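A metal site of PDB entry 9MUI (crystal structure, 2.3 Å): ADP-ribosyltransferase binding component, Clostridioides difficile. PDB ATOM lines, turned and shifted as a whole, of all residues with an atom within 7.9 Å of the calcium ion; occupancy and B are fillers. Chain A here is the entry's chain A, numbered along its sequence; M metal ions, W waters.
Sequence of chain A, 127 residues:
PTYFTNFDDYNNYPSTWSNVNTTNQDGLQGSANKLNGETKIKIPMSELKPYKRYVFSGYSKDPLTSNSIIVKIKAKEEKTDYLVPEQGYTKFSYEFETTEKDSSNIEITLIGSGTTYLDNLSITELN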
ATOM      1  N   PHE A   4      39.551 -29.556  -6.245  1.00  0.00           N
ATOM      2  CA  PHE A   4      38.154 -29.202  -6.141  1.00  0.00           C
ATOM      3  C   PHE A   4      37.980 -27.701  -6.302  1.00  0.00           C
ATOM      4  O   PHE A   4      38.849 -26.918  -5.890  1.00  0.00           O
ATOM      5  CB  PHE A   4      37.560 -29.660  -4.812  1.00  0.00           C
ATOM      6  CG  PHE A   4      36.075 -29.390  -4.659  1.00  0.00           C
ATOM      7  CD1 PHE A   4      35.139 -30.194  -5.283  1.00  0.00           C
ATOM      8  CD2 PHE A   4      35.631 -28.327  -3.876  1.00  0.00           C
ATOM      9  CE1 PHE A   4      33.768 -29.962  -5.139  1.00  0.00           C
ATOM     10  CE2 PHE A   4      34.264 -28.085  -3.732  1.00  0.00           C
ATOM     11  CZ  PHE A   4      33.334 -28.904  -4.384  1.00  0.00           C
ATOM     12  N   THR A   5      36.887 -27.298  -6.958  1.00  0.00           N
ATOM     13  CA  THR A   5      36.443 -25.920  -6.924  1.00  0.00           C
ATOM     14  C   THR A   5      34.924 -25.906  -6.857  1.00  0.00           C
ATOM     15  O   THR A   5      34.244 -26.751  -7.452  1.00  0.00           O
ATOM     16  CB  THR A   5      36.955 -25.091  -8.129  1.00  0.00           C
ATOM     17  OG1 THR A   5      36.482 -23.740  -8.014  1.00  0.00           O
ATOM     18  CG2 THR A   5      36.497 -25.660  -9.475  1.00  0.00           C
ATOM     19  N   ASN A   6      34.399 -24.964  -6.072  1.00  0.00           N
ATOM     20  CA  ASN A   6      32.965 -24.724  -5.960  1.00  0.00           C
ATOM     21  C   ASN A   6      32.578 -23.403  -6.625  1.00  0.00           C
ATOM     22  O   ASN A   6      31.440 -22.949  -6.449  1.00  0.00           O
ATOM     23  CB  ASN A   6      32.513 -24.726  -4.499  1.00  0.00           C
ATOM     24  CG  ASN A   6      33.277 -23.724  -3.624  1.00  0.00           C
ATOM     25  OD1 ASN A   6      33.881 -22.758  -4.104  1.00  0.00           O
ATOM     26  ND2 ASN A   6      33.254 -23.960  -2.330  1.00  0.00           N
ATOM     27  N   PHE A   7      33.504 -22.775  -7.334  1.00  0.00           N
ATOM     28  CA  PHE A   7      33.291 -21.501  -7.995  1.00  0.00           C
ATOM     29  C   PHE A   7      32.801 -20.423  -7.027  1.00  0.00           C
ATOM     30  O   PHE A   7      32.213 -19.423  -7.428  1.00  0.00           O
ATOM     31  CB  PHE A   7      32.349 -21.662  -9.189  1.00  0.00           C
ATOM     32  CG  PHE A   7      32.872 -22.608 -10.254  1.00  0.00           C
ATOM     33  CD1 PHE A   7      33.982 -22.265 -11.023  1.00  0.00           C
ATOM     34  CD2 PHE A   7      32.289 -23.862 -10.446  1.00  0.00           C
ATOM     35  CE1 PHE A   7      34.493 -23.138 -11.975  1.00  0.00           C
ATOM     36  CE2 PHE A   7      32.785 -24.740 -11.392  1.00  0.00           C
ATOM     37  CZ  PHE A   7      33.892 -24.375 -12.166  1.00  0.00           C
ATOM     38  N   ASP A   8      33.108 -20.608  -5.735  1.00  0.00           N
ATOM     39  CA  ASP A   8      32.752 -19.665  -4.699  1.00  0.00           C
ATOM     40  C   ASP A   8      34.032 -19.312  -3.935  1.00  0.00           C
ATOM     41  O   ASP A   8      34.868 -18.560  -4.460  1.00  0.00           O
ATOM     42  CB  ASP A   8      31.641 -20.287  -3.830  1.00  0.00           C
ATOM     43  CG  ASP A   8      30.308 -20.391  -4.579  1.00  0.00           C
ATOM     44  OD1 ASP A   8      29.892 -19.360  -5.140  1.00  0.00           O
ATOM     45  OD2 ASP A   8      29.674 -21.481  -4.602  1.00  0.00           O
ATOM     46  N   ASP A   9      34.228 -19.856  -2.749  1.00  0.00           N
ATOM     47  CA  ASP A   9      35.386 -19.544  -1.934  1.00  0.00           C
ATOM     48  C   ASP A   9      36.551 -20.504  -2.145  1.00  0.00           C
ATOM     49  O   ASP A   9      37.680 -20.125  -1.800  1.00  0.00           O
ATOM     50  CB  ASP A   9      35.032 -19.599  -0.452  1.00  0.00           C
ATOM     51  CG  ASP A   9      34.523 -20.968  -0.043  1.00  0.00           C
ATOM     52  OD1 ASP A   9      33.667 -21.511  -0.780  1.00  0.00           O
ATOM     53  OD2 ASP A   9      35.015 -21.534   0.969  1.00  0.00           O
ATOM     54  N   THR A  22      31.452 -16.610 -13.094  1.00  0.00           N
ATOM     55  CA  THR A  22      30.755 -16.945 -11.864  1.00  0.00           C
ATOM     56  C   THR A  22      29.925 -15.782 -11.327  1.00  0.00           C
ATOM     57  O   THR A  22      29.593 -15.764 -10.127  1.00  0.00           O
ATOM     58  CB  THR A  22      31.740 -17.404 -10.776  1.00  0.00           C
ATOM     59  OG1 THR A  22      32.683 -16.359 -10.521  1.00  0.00           O
ATOM     60  CG2 THR A  22      32.495 -18.674 -11.203  1.00  0.00           C
ATOM     61  N   ASN A  24      26.906 -15.048 -11.060  1.00  0.00           N
ATOM     62  CA  ASN A  24      25.557 -15.588 -11.056  1.00  0.00           C
ATOM     63  C   ASN A  24      25.317 -16.245  -9.701  1.00  0.00           C
ATOM     64  O   ASN A  24      26.243 -16.449  -8.922  1.00  0.00           O
ATOM     65  CB  ASN A  24      25.354 -16.587 -12.189  1.00  0.00           C
ATOM     66  CG  ASN A  24      26.248 -17.849 -12.057  1.00  0.00           C
ATOM     67  OD1 ASN A  24      25.948 -18.762 -11.289  1.00  0.00           O
ATOM     68  ND2 ASN A  24      27.354 -17.871 -12.787  1.00  0.00           N
ATOM     69  N   ASP A  26      23.407 -19.229  -9.587  1.00  0.00           N
ATOM     70  CA  ASP A  26      22.802 -20.423 -10.161  1.00  0.00           C
ATOM     71  C   ASP A  26      23.562 -21.715  -9.823  1.00  0.00           C
ATOM     72  O   ASP A  26      23.395 -22.712 -10.537  1.00  0.00           O
ATOM     73  CB  ASP A  26      22.729 -20.285 -11.686  1.00  0.00           C
ATOM     74  CG  ASP A  26      21.844 -19.149 -12.137  1.00  0.00           C
ATOM     75  OD1 ASP A  26      20.614 -19.313 -12.059  1.00  0.00           O
ATOM     76  OD2 ASP A  26      22.372 -18.102 -12.560  1.00  0.00           O
ATOM     77  N   GLY A  27      24.452 -21.694  -8.805  1.00  0.00           N
ATOM     78  CA  GLY A  27      25.234 -22.868  -8.490  1.00  0.00           C
ATOM     79  C   GLY A  27      24.425 -23.944  -7.773  1.00  0.00           C
ATOM     80  O   GLY A  27      23.293 -23.699  -7.346  1.00  0.00           O
ATOM     81  N   LEU A  28      25.003 -25.148  -7.673  1.00  0.00           N
ATOM     82  CA  LEU A  28      24.497 -26.130  -6.718  1.00  0.00           C
ATOM     83  C   LEU A  28      24.428 -25.513  -5.326  1.00  0.00           C
ATOM     84  O   LEU A  28      23.438 -25.677  -4.610  1.00  0.00           O
ATOM     85  CB  LEU A  28      25.370 -27.392  -6.700  1.00  0.00           C
ATOM     86  CG  LEU A  28      24.731 -28.659  -6.139  1.00  0.00           C
ATOM     87  CD1 LEU A  28      23.332 -28.927  -6.648  1.00  0.00           C
ATOM     88  CD2 LEU A  28      25.610 -29.856  -6.429  1.00  0.00           C
ATOM     89  N   GLN A  29      25.476 -24.809  -4.924  1.00  0.00           N
ATOM     90  CA  GLN A  29      25.430 -23.869  -3.825  1.00  0.00           C
ATOM     91  C   GLN A  29      26.130 -22.608  -4.321  1.00  0.00           C
ATOM     92  O   GLN A  29      27.071 -22.706  -5.117  1.00  0.00           O
ATOM     93  CB  GLN A  29      26.118 -24.422  -2.565  1.00  0.00           C
ATOM     94  CG  GLN A  29      25.660 -25.819  -2.166  1.00  0.00           C
ATOM     95  CD  GLN A  29      26.518 -26.942  -2.744  1.00  0.00           C
ATOM     96  OE1 GLN A  29      27.619 -26.717  -3.240  1.00  0.00           O
ATOM     97  NE2 GLN A  29      26.014 -28.174  -2.667  1.00  0.00           N
ATOM     98  N   GLY A  30      25.661 -21.442  -3.906  1.00  0.00           N
ATOM     99  CA  GLY A  30      26.318 -20.217  -4.347  1.00  0.00           C
ATOM    100  C   GLY A  30      26.329 -20.011  -5.866  1.00  0.00           C
ATOM    101  O   GLY A  30      25.305 -20.106  -6.543  1.00  0.00           O
ATOM    102  N   SER A  31      27.518 -19.691  -6.400  1.00  0.00           N
ATOM    103  CA  SER A  31      27.721 -19.416  -7.811  1.00  0.00           C
ATOM    104  C   SER A  31      28.082 -20.703  -8.585  1.00  0.00           C
ATOM    105  O   SER A  31      28.622 -21.669  -8.035  1.00  0.00           O
ATOM    106  CB  SER A  31      28.841 -18.390  -7.996  1.00  0.00           C
ATOM    107  OG  SER A  31      28.461 -17.114  -7.548  1.00  0.00           O
ATOM    108  N   ALA A  32      27.777 -20.667  -9.883  1.00  0.00           N
ATOM    109  CA  ALA A  32      28.164 -21.680 -10.854  1.00  0.00           C
ATOM    110  C   ALA A  32      29.124 -21.080 -11.868  1.00  0.00           C
ATOM    111  O   ALA A  32      29.225 -19.846 -11.997  1.00  0.00           O
ATOM    112  CB  ALA A  32      26.933 -22.237 -11.589  1.00  0.00           C
ATOM    113  N   ASN A  33      29.854 -21.938 -12.598  1.00  0.00           N
ATOM    114  CA  ASN A  33      30.477 -21.495 -13.839  1.00  0.00           C
ATOM    115  C   ASN A  33      29.398 -21.521 -14.921  1.00  0.00           C
ATOM    116  O   ASN A  33      28.920 -22.598 -15.300  1.00  0.00           O
ATOM    117  CB  ASN A  33      31.680 -22.342 -14.259  1.00  0.00           C
ATOM    118  CG  ASN A  33      32.374 -21.786 -15.538  1.00  0.00           C
ATOM    119  OD1 ASN A  33      32.107 -20.639 -15.962  1.00  0.00           O
ATOM    120  ND2 ASN A  33      33.232 -22.584 -16.149  1.00  0.00           N
ATOM    121  N   TYR A  89      20.393 -29.958 -11.440  1.00  0.00           N
ATOM    122  CA  TYR A  89      21.760 -30.439 -11.341  1.00  0.00           C
ATOM    123  C   TYR A  89      21.801 -31.948 -11.160  1.00  0.00           C
ATOM    124  O   TYR A  89      21.060 -32.493 -10.348  1.00  0.00           O
ATOM    125  CB  TYR A  89      22.473 -29.773 -10.171  1.00  0.00           C
ATOM    126  CG  TYR A  89      23.116 -28.464 -10.513  1.00  0.00           C
ATOM    127  CD1 TYR A  89      24.220 -28.397 -11.366  1.00  0.00           C
ATOM    128  CD2 TYR A  89      22.650 -27.301  -9.937  1.00  0.00           C
ATOM    129  CE1 TYR A  89      24.821 -27.177 -11.643  1.00  0.00           C
ATOM    130  CE2 TYR A  89      23.222 -26.090 -10.201  1.00  0.00           C
ATOM    131  CZ  TYR A  89      24.301 -26.026 -11.051  1.00  0.00           C
ATOM    132  OH  TYR A  89      24.859 -24.809 -11.278  1.00  0.00           O
ATOM    133  N   LEU A 118      27.839 -25.209 -14.622  1.00  0.00           N
ATOM    134  CA  LEU A 118      28.747 -26.199 -14.060  1.00  0.00           C
ATOM    135  C   LEU A 118      29.061 -25.810 -12.626  1.00  0.00           C
ATOM    136  O   LEU A 118      29.283 -24.634 -12.341  1.00  0.00           O
ATOM    137  CB  LEU A 118      30.045 -26.266 -14.856  1.00  0.00           C
ATOM    138  CG  LEU A 118      30.048 -26.707 -16.312  1.00  0.00           C
ATOM    139  CD1 LEU A 118      31.479 -26.511 -16.904  1.00  0.00           C
ATOM    140  CD2 LEU A 118      29.573 -28.169 -16.400  1.00  0.00           C
ATOM    141  N   ASP A 119      29.114 -26.798 -11.736  1.00  0.00           N
ATOM    142  CA  ASP A 119      29.510 -26.544 -10.359  1.00  0.00           C
ATOM    143  C   ASP A 119      30.229 -27.744  -9.762  1.00  0.00           C
ATOM    144  O   ASP A 119      30.095 -28.876 -10.238  1.00  0.00           O
ATOM    145  CB  ASP A 119      28.315 -26.179  -9.481  1.00  0.00           C
ATOM    146  CG  ASP A 119      28.700 -25.190  -8.391  1.00  0.00           C
ATOM    147  OD1 ASP A 119      29.912 -24.892  -8.262  1.00  0.00           O
ATOM    148  OD2 ASP A 119      27.802 -24.721  -7.675  1.00  0.00           O
ATOM    149  N   ASN A 120      31.026 -27.450  -8.725  1.00  0.00           N
ATOM    150  CA  ASN A 120      31.714 -28.438  -7.885  1.00  0.00           C
ATOM    151  C   ASN A 120      32.500 -29.467  -8.717  1.00  0.00           C
ATOM    152  O   ASN A 120      32.282 -30.665  -8.633  1.00  0.00           O
ATOM    153  CB  ASN A 120      30.737 -29.151  -6.944  1.00  0.00           C
ATOM    154  CG  ASN A 120      30.095 -28.200  -5.910  1.00  0.00           C
ATOM    155  OD1 ASN A 120      30.409 -27.003  -5.843  1.00  0.00           O
ATOM    156  ND2 ASN A 120      29.182 -28.743  -5.115  1.00  0.00           N
HETATM  157 CA    CA M   1      29.084 -23.135  -6.336  1.00  0.00          CA
HETATM  158  O   HOH W   1      29.222 -24.829  -4.955  1.00  0.00           O
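The side-chain hydroxyl (OG) of Ser 31 lies within hydrogen-bond range of the backbone carbonyl oxygen (O) of Asn 24 (2.7 Å). The side-chain hydroxyl (OG) of Ser 31 is in hydrogen-bond range of the backbone carbonyl oxygen (O) of Thr 22, at 3.1 Å. OD1 of Asp 9 is in hydrogen-bond range of ND2 of Asn 6. OE1 of Gln 29 sits at hydrogen-bond distance from ND2 of Asn 120, 3.2 Å away. The side-chain amide oxygen of Asn 120 lies close to the side-chain carboxylate of Asp 119. OD2 of Asp 119 sits close to N of Leu 28 (2.8 Å).
The nearest printed residue that does not touch the calcium ion is Asn 120 (4.1 Å).
The calcium ion is bound by water W1 (2.2 Å), the backbone carbonyl oxygen (O) of Ser 31 (2.3 Å), the backbone carbonyl oxygen (O) of Asn 6 (2.4 Å), the backbone carbonyl oxygen (O) of Gln 29 (2.4 Å), the side-chain carboxylate (OD2) of Asp 119 (2.4 Å), the side-chain carboxylate (OD2) of Asp 8 (2.5 Å) and the side-chain carboxylate (OD1) of Asp 119 (2.7 Å).
Water W1 lies within hydrogen-bond range of OD1 of Asn 120 (2.6 Å) and OE1 of Gln 29 (3.0 Å).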
